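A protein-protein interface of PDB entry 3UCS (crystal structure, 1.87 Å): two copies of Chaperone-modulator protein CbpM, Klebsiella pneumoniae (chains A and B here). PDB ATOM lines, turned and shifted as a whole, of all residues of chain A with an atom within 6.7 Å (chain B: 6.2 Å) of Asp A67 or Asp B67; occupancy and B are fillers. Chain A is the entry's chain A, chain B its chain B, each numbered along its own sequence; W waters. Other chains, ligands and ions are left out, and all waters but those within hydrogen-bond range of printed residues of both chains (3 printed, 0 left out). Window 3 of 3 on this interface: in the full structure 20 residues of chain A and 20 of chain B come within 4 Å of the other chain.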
ATOM      1  N   GLU A  27      31.358   3.529 -10.333  1.00  0.00           N
ATOM      2  CA  GLU A  27      30.326   2.639  -9.761  1.00  0.00           C
ATOM      3  C   GLU A  27      29.389   2.097 -10.855  1.00  0.00           C
ATOM      4  O   GLU A  27      29.043   0.916 -10.879  1.00  0.00           O
ATOM      5  CB  GLU A  27      29.498   3.340  -8.674  1.00  0.00           C
ATOM      6  CG  GLU A  27      28.542   2.333  -7.940  1.00  0.00           C
ATOM      7  CD  GLU A  27      27.543   2.957  -6.975  1.00  0.00           C
ATOM      8  OE1 GLU A  27      27.340   4.188  -7.025  1.00  0.00           O
ATOM      9  OE2 GLU A  27      26.948   2.187  -6.173  1.00  0.00           O
ATOM     10  N   LEU A  31      28.737  -1.749 -11.652  1.00  0.00           N
ATOM     11  CA  LEU A  31      27.398  -2.322 -11.622  1.00  0.00           C
ATOM     12  C   LEU A  31      27.047  -2.999 -12.937  1.00  0.00           C
ATOM     13  O   LEU A  31      25.966  -3.572 -13.067  1.00  0.00           O
ATOM     14  CB  LEU A  31      26.359  -1.240 -11.263  1.00  0.00           C
ATOM     15  CG  LEU A  31      26.460  -0.719  -9.822  1.00  0.00           C
ATOM     16  CD1 LEU A  31      25.660   0.597  -9.577  1.00  0.00           C
ATOM     17  CD2 LEU A  31      25.968  -1.822  -8.836  1.00  0.00           C
ATOM     18  N   ARG A  61      17.094   8.446 -12.560  1.00  0.00           N
ATOM     19  CA  ARG A  61      17.477   8.938 -11.233  1.00  0.00           C
ATOM     20  C   ARG A  61      16.681  10.205 -10.880  1.00  0.00           C
ATOM     21  O   ARG A  61      16.226  10.352  -9.751  1.00  0.00           O
ATOM     22  CB  ARG A  61      18.963   9.249 -11.130  1.00  0.00           C
ATOM     23  CG  ARG A  61      19.336   9.799  -9.710  1.00  0.00           C
ATOM     24  CD  ARG A  61      20.751  10.390  -9.595  1.00  0.00           C
ATOM     25  NE  ARG A  61      21.017  11.557 -10.453  1.00  0.00           N
ATOM     26  CZ  ARG A  61      22.244  12.062 -10.672  1.00  0.00           C
ATOM     27  NH1 ARG A  61      23.313  11.531 -10.075  1.00  0.00           N
ATOM     28  NH2 ARG A  61      22.419  13.103 -11.479  1.00  0.00           N
ATOM     29  N   GLU A  65      14.525   9.026  -8.066  1.00  0.00           N
ATOM     30  CA  GLU A  65      15.503   9.274  -7.018  1.00  0.00           C
ATOM     31  C   GLU A  65      16.017   7.998  -6.360  1.00  0.00           C
ATOM     32  O   GLU A  65      15.942   7.847  -5.137  1.00  0.00           O
ATOM     33  CB  GLU A  65      14.962  10.258  -5.984  1.00  0.00           C
ATOM     34  CG  GLU A  65      14.990  11.698  -6.471  1.00  0.00           C
ATOM     35  CD  GLU A  65      16.403  12.277  -6.616  1.00  0.00           C
ATOM     36  OE1 GLU A  65      17.397  11.675  -6.138  1.00  0.00           O
ATOM     37  OE2 GLU A  65      16.512  13.339  -7.252  1.00  0.00           O
ATOM     38  N   LEU A  66      16.494   7.069  -7.177  1.00  0.00           N
ATOM     39  CA  LEU A  66      17.143   5.868  -6.655  1.00  0.00           C
ATOM     40  C   LEU A  66      18.653   6.037  -6.770  1.00  0.00           C
ATOM     41  O   LEU A  66      19.127   6.701  -7.693  1.00  0.00           O
ATOM     42  CB  LEU A  66      16.720   4.617  -7.444  1.00  0.00           C
ATOM     43  CG  LEU A  66      15.200   4.393  -7.527  1.00  0.00           C
ATOM     44  CD1 LEU A  66      14.859   3.090  -8.263  1.00  0.00           C
ATOM     45  CD2 LEU A  66      14.547   4.379  -6.150  1.00  0.00           C
ATOM     46  N   ASP A  67      19.396   5.391  -5.875  1.00  0.00           N
ATOM     47  CA  ASP A  67      20.851   5.265  -6.026  1.00  0.00           C
ATOM     48  C   ASP A  67      21.169   4.354  -7.214  1.00  0.00           C
ATOM     49  O   ASP A  67      20.274   3.666  -7.719  1.00  0.00           O
ATOM     50  CB  ASP A  67      21.494   4.736  -4.727  1.00  0.00           C
ATOM     51  CG  ASP A  67      21.147   3.266  -4.418  1.00  0.00           C
ATOM     52  OD1 ASP A  67      21.635   2.763  -3.365  1.00  0.00           O
ATOM     53  OD2 ASP A  67      20.417   2.597  -5.201  1.00  0.00           O
ATOM     54  N   TRP A  68      22.415   4.341  -7.665  1.00  0.00           N
ATOM     55  CA  TRP A  68      22.732   3.638  -8.927  1.00  0.00           C
ATOM     56  C   TRP A  68      22.421   2.123  -8.928  1.00  0.00           C
ATOM     57  O   TRP A  68      21.942   1.596  -9.937  1.00  0.00           O
ATOM     58  CB  TRP A  68      24.170   3.904  -9.385  1.00  0.00           C
ATOM     59  CG  TRP A  68      24.450   5.357  -9.688  1.00  0.00           C
ATOM     60  CD1 TRP A  68      25.379   6.160  -9.086  1.00  0.00           C
ATOM     61  CD2 TRP A  68      23.787   6.173 -10.667  1.00  0.00           C
ATOM     62  NE1 TRP A  68      25.335   7.432  -9.632  1.00  0.00           N
ATOM     63  CE2 TRP A  68      24.362   7.465 -10.599  1.00  0.00           C
ATOM     64  CE3 TRP A  68      22.761   5.935 -11.595  1.00  0.00           C
ATOM     65  CZ2 TRP A  68      23.955   8.513 -11.431  1.00  0.00           C
ATOM     66  CZ3 TRP A  68      22.332   6.981 -12.408  1.00  0.00           C
ATOM     67  CH2 TRP A  68      22.938   8.266 -12.318  1.00  0.00           C
ATOM     68  N   PRO A  69      22.684   1.410  -7.820  1.00  0.00           N
ATOM     69  CA  PRO A  69      22.293  -0.009  -7.887  1.00  0.00           C
ATOM     70  C   PRO A  69      20.780  -0.190  -8.165  1.00  0.00           C
ATOM     71  O   PRO A  69      20.383  -1.097  -8.914  1.00  0.00           O
ATOM     72  CB  PRO A  69      22.629  -0.530  -6.469  1.00  0.00           C
ATOM     73  CG  PRO A  69      23.814   0.349  -6.033  1.00  0.00           C
ATOM     74  CD  PRO A  69      23.425   1.732  -6.579  1.00  0.00           C
ATOM     75  N   GLY A  70      19.954   0.652  -7.560  1.00  0.00           N
ATOM     76  CA  GLY A  70      18.485   0.541  -7.711  1.00  0.00           C
ATOM     77  C   GLY A  70      18.074   0.947  -9.133  1.00  0.00           C
ATOM     78  O   GLY A  70      17.160   0.374  -9.715  1.00  0.00           O
ATOM     79  N   ILE A  71      18.740   1.968  -9.672  1.00  0.00           N
ATOM     80  CA  ILE A  71      18.533   2.348 -11.074  1.00  0.00           C
ATOM     81  C   ILE A  71      18.891   1.197 -12.029  1.00  0.00           C
ATOM     82  O   ILE A  71      18.129   0.914 -12.939  1.00  0.00           O
ATOM     83  CB  ILE A  71      19.385   3.603 -11.468  1.00  0.00           C
ATOM     84  CG1 ILE A  71      18.944   4.851 -10.693  1.00  0.00           C
ATOM     85  CG2 ILE A  71      19.331   3.861 -12.990  1.00  0.00           C
ATOM     86  CD1 ILE A  71      17.527   5.338 -10.964  1.00  0.00           C
ATOM     87  N   ALA A  72      20.043   0.546 -11.845  1.00  0.00           N
ATOM     88  CA  ALA A  72      20.408  -0.544 -12.730  1.00  0.00           C
ATOM     89  C   ALA A  72      19.306  -1.617 -12.808  1.00  0.00           C
ATOM     90  O   ALA A  72      18.903  -2.046 -13.916  1.00  0.00           O
ATOM     91  CB  ALA A  72      21.700  -1.176 -12.282  1.00  0.00           C
ATOM     92  N   GLU B  27      11.546   4.478   7.255  1.00  0.00           N
ATOM     93  CA  GLU B  27      11.749   4.692   5.812  1.00  0.00           C
ATOM     94  C   GLU B  27      10.819   3.808   4.966  1.00  0.00           C
ATOM     95  O   GLU B  27      10.246   4.273   3.978  1.00  0.00           O
ATOM     96  CB  GLU B  27      13.202   4.453   5.419  1.00  0.00           C
ATOM     97  CG  GLU B  27      13.466   4.863   3.952  1.00  0.00           C
ATOM     98  CD  GLU B  27      14.854   4.555   3.434  1.00  0.00           C
ATOM     99  OE1 GLU B  27      15.591   3.735   4.039  1.00  0.00           O
ATOM    100  OE2 GLU B  27      15.208   5.141   2.385  1.00  0.00           O
ATOM    101  N   ARG B  61      16.063  -7.422  -0.540  1.00  0.00           N
ATOM    102  CA  ARG B  61      17.230  -6.621  -0.151  1.00  0.00           C
ATOM    103  C   ARG B  61      18.464  -7.514  -0.074  1.00  0.00           C
ATOM    104  O   ARG B  61      19.526  -7.161  -0.582  1.00  0.00           O
ATOM    105  CB  ARG B  61      17.012  -5.869   1.191  1.00  0.00           C
ATOM    106  CG  ARG B  61      18.323  -5.168   1.690  1.00  0.00           C
ATOM    107  CD  ARG B  61      18.452  -5.048   3.205  1.00  0.00           C
ATOM    108  NE  ARG B  61      18.788  -6.314   3.862  1.00  0.00           N
ATOM    109  CZ  ARG B  61      18.558  -6.565   5.159  1.00  0.00           C
ATOM    110  NH1 ARG B  61      17.995  -5.637   5.937  1.00  0.00           N
ATOM    111  NH2 ARG B  61      18.886  -7.738   5.692  1.00  0.00           N
ATOM    112  N   GLU B  65      20.790  -6.848  -2.910  1.00  0.00           N
ATOM    113  CA  GLU B  65      21.558  -5.806  -2.199  1.00  0.00           C
ATOM    114  C   GLU B  65      21.265  -4.372  -2.673  1.00  0.00           C
ATOM    115  O   GLU B  65      22.170  -3.611  -3.064  1.00  0.00           O
ATOM    116  CB  GLU B  65      23.066  -6.109  -2.205  1.00  0.00           C
ATOM    117  CG  GLU B  65      23.484  -7.207  -1.204  1.00  0.00           C
ATOM    118  CD  GLU B  65      23.410  -6.728   0.246  1.00  0.00           C
ATOM    119  OE1 GLU B  65      23.259  -5.504   0.462  1.00  0.00           O
ATOM    120  OE2 GLU B  65      23.480  -7.575   1.164  1.00  0.00           O
ATOM    121  N   LEU B  66      19.986  -4.023  -2.641  1.00  0.00           N
ATOM    122  CA  LEU B  66      19.548  -2.661  -2.913  1.00  0.00           C
ATOM    123  C   LEU B  66      19.097  -1.986  -1.622  1.00  0.00           C
ATOM    124  O   LEU B  66      18.582  -2.667  -0.728  1.00  0.00           O
ATOM    125  CB  LEU B  66      18.370  -2.686  -3.893  1.00  0.00           C
ATOM    126  CG  LEU B  66      18.511  -3.437  -5.233  1.00  0.00           C
ATOM    127  CD1 LEU B  66      17.291  -3.252  -6.130  1.00  0.00           C
ATOM    128  CD2 LEU B  66      19.774  -2.962  -5.979  1.00  0.00           C
ATOM    129  N   ASP B  67      19.259  -0.656  -1.544  1.00  0.00           N
ATOM    130  CA  ASP B  67      18.654   0.148  -0.466  1.00  0.00           C
ATOM    131  C   ASP B  67      17.134   0.126  -0.623  1.00  0.00           C
ATOM    132  O   ASP B  67      16.611  -0.251  -1.678  1.00  0.00           O
ATOM    133  CB  ASP B  67      19.150   1.593  -0.520  1.00  0.00           C
ATOM    134  CG  ASP B  67      18.954   2.359   0.804  1.00  0.00           C
ATOM    135  OD1 ASP B  67      19.389   3.528   0.849  1.00  0.00           O
ATOM    136  OD2 ASP B  67      18.374   1.835   1.793  1.00  0.00           O
ATOM    137  N   TRP B  68      16.436   0.545   0.417  1.00  0.00           N
ATOM    138  CA  TRP B  68      14.972   0.431   0.447  1.00  0.00           C
ATOM    139  C   TRP B  68      14.229   1.132  -0.702  1.00  0.00           C
ATOM    140  O   TRP B  68      13.278   0.574  -1.215  1.00  0.00           O
ATOM    141  CB  TRP B  68      14.424   0.843   1.819  1.00  0.00           C
ATOM    142  CG  TRP B  68      14.909  -0.069   2.924  1.00  0.00           C
ATOM    143  CD1 TRP B  68      15.720   0.266   3.971  1.00  0.00           C
ATOM    144  CD2 TRP B  68      14.652  -1.482   3.047  1.00  0.00           C
ATOM    145  NE1 TRP B  68      15.947  -0.850   4.765  1.00  0.00           N
ATOM    146  CE2 TRP B  68      15.304  -1.927   4.220  1.00  0.00           C
ATOM    147  CE3 TRP B  68      13.906  -2.403   2.295  1.00  0.00           C
ATOM    148  CZ2 TRP B  68      15.248  -3.269   4.653  1.00  0.00           C
ATOM    149  CZ3 TRP B  68      13.861  -3.748   2.727  1.00  0.00           C
ATOM    150  CH2 TRP B  68      14.524  -4.153   3.894  1.00  0.00           C
ATOM    151  N   PRO B  69      14.670   2.328  -1.136  1.00  0.00           N
ATOM    152  CA  PRO B  69      13.913   2.905  -2.264  1.00  0.00           C
ATOM    153  C   PRO B  69      14.007   2.043  -3.530  1.00  0.00           C
ATOM    154  O   PRO B  69      13.024   1.930  -4.258  1.00  0.00           O
ATOM    155  CB  PRO B  69      14.576   4.278  -2.484  1.00  0.00           C
ATOM    156  CG  PRO B  69      15.018   4.672  -1.097  1.00  0.00           C
ATOM    157  CD  PRO B  69      15.538   3.335  -0.490  1.00  0.00           C
ATOM    158  N   GLY B  70      15.169   1.440  -3.769  1.00  0.00           N
ATOM    159  CA  GLY B  70      15.363   0.564  -4.930  1.00  0.00           C
ATOM    160  C   GLY B  70      14.570  -0.727  -4.821  1.00  0.00           C
ATOM    161  O   GLY B  70      14.082  -1.247  -5.828  1.00  0.00           O
ATOM    162  N   ILE B  71      14.445  -1.240  -3.594  1.00  0.00           N
ATOM    163  CA  ILE B  71      13.629  -2.412  -3.323  1.00  0.00           C
ATOM    164  C   ILE B  71      12.156  -2.150  -3.568  1.00  0.00           C
ATOM    165  O   ILE B  71      11.499  -2.972  -4.191  1.00  0.00           O
ATOM    166  CB  ILE B  71      13.832  -2.971  -1.866  1.00  0.00           C
ATOM    167  CG1 ILE B  71      15.262  -3.490  -1.703  1.00  0.00           C
ATOM    168  CG2 ILE B  71      12.798  -4.066  -1.542  1.00  0.00           C
ATOM    169  CD1 ILE B  71      15.636  -4.655  -2.682  1.00  0.00           C
ATOM    170  N   ALA B  72      11.648  -1.010  -3.114  1.00  0.00           N
ATOM    171  CA  ALA B  72      10.241  -0.657  -3.306  1.00  0.00           C
ATOM    172  C   ALA B  72       9.915  -0.647  -4.805  1.00  0.00           C
ATOM    173  O   ALA B  72       8.900  -1.216  -5.243  1.00  0.00           O
ATOM    174  CB  ALA B  72       9.950   0.721  -2.698  1.00  0.00           C
HETATM  175  O   HOH W   1      18.420   1.219  -4.360  1.00  0.00           O
HETATM  176  O   HOH W   2      14.855  -1.025  -8.581  1.00  0.00           O
HETATM  177  O   HOH W   3      21.210   0.191  -3.311  1.00  0.00           O
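N of Gly A70 lies within hydrogen-bond range of OD2 of Asp A67.
Among the printed residues, merely in contact across the chains: Leu A66 with Pro B69 (3.4 Å), Pro A69 with Leu B66 (3.5 Å), Leu A66 with Gly B70 (3.8 Å), Gly A70 with Leu B66 (3.9 Å) and Asp A67 with Asp B67 (3.95 Å).
Of the printed residues of chain B, Asp A67 touches Asp B67.
Printed residues of chain A within 4 Å of Asp B67: Asp A67 (3.95 Å).
Of the printed residues of chain B, Pro A69 touches Leu B66.
Printed residues of chain B within 4 Å of Gly A70: Leu B66 (3.9 Å).
Printed residues of chain A within 4 Å of Pro B69: Leu A66 (3.4 Å).
The nearest printed residue of chain B that does not touch Asp A67 is Gly B70 (5.5 Å).
The nearest printed residue of chain A that does not touch Asp B67 is Pro A69 (6.0 Å).
Of the 11 printed residues of chain A, 4 touch a printed residue of chain B.
Hydrophobic or aromatic side chains of chain A within 4 Å of the printed part of chain B: Leu A66 and Pro A69.
Of the 10 printed residues of chain B, 4 touch a printed residue of chain A.
Printed residues of chain B that touch a printed residue of chain A: Leu B66, Asp B67, Pro B69 and Gly B70.
Leu A66 touches Pro B69, and with the chains exchanged Pro A69 touches Leu B66.
Leu A66 touches Gly B70, and with the chains exchanged Gly A70 touches Leu B66.
Asp A67 touches its own counterpart, Asp B67.
Positions printed for both chains: 27, 61, 65, 66, 67, 68, 69, 70, 71 and 72.
Of the 5 pairs that touch across the chains among the printed residues, 5 have their exchanged pair printed and touching as well.
Water W1 lies within hydrogen-bond range of OD2 of Asp A67 (2.6 Å), N of Gly B70 (3.3 Å) and N of Asp B67 (3.5 Å).
Water W3 lies within hydrogen-bond range of the side-chain carboxylate of Asp A67 (2.6 Å) and the backbone NH of Asp B67 (2.8 Å).
Water W2 bridges O of Gly B70 (2.9 Å) and O of Gly A70 (2.9 Å).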
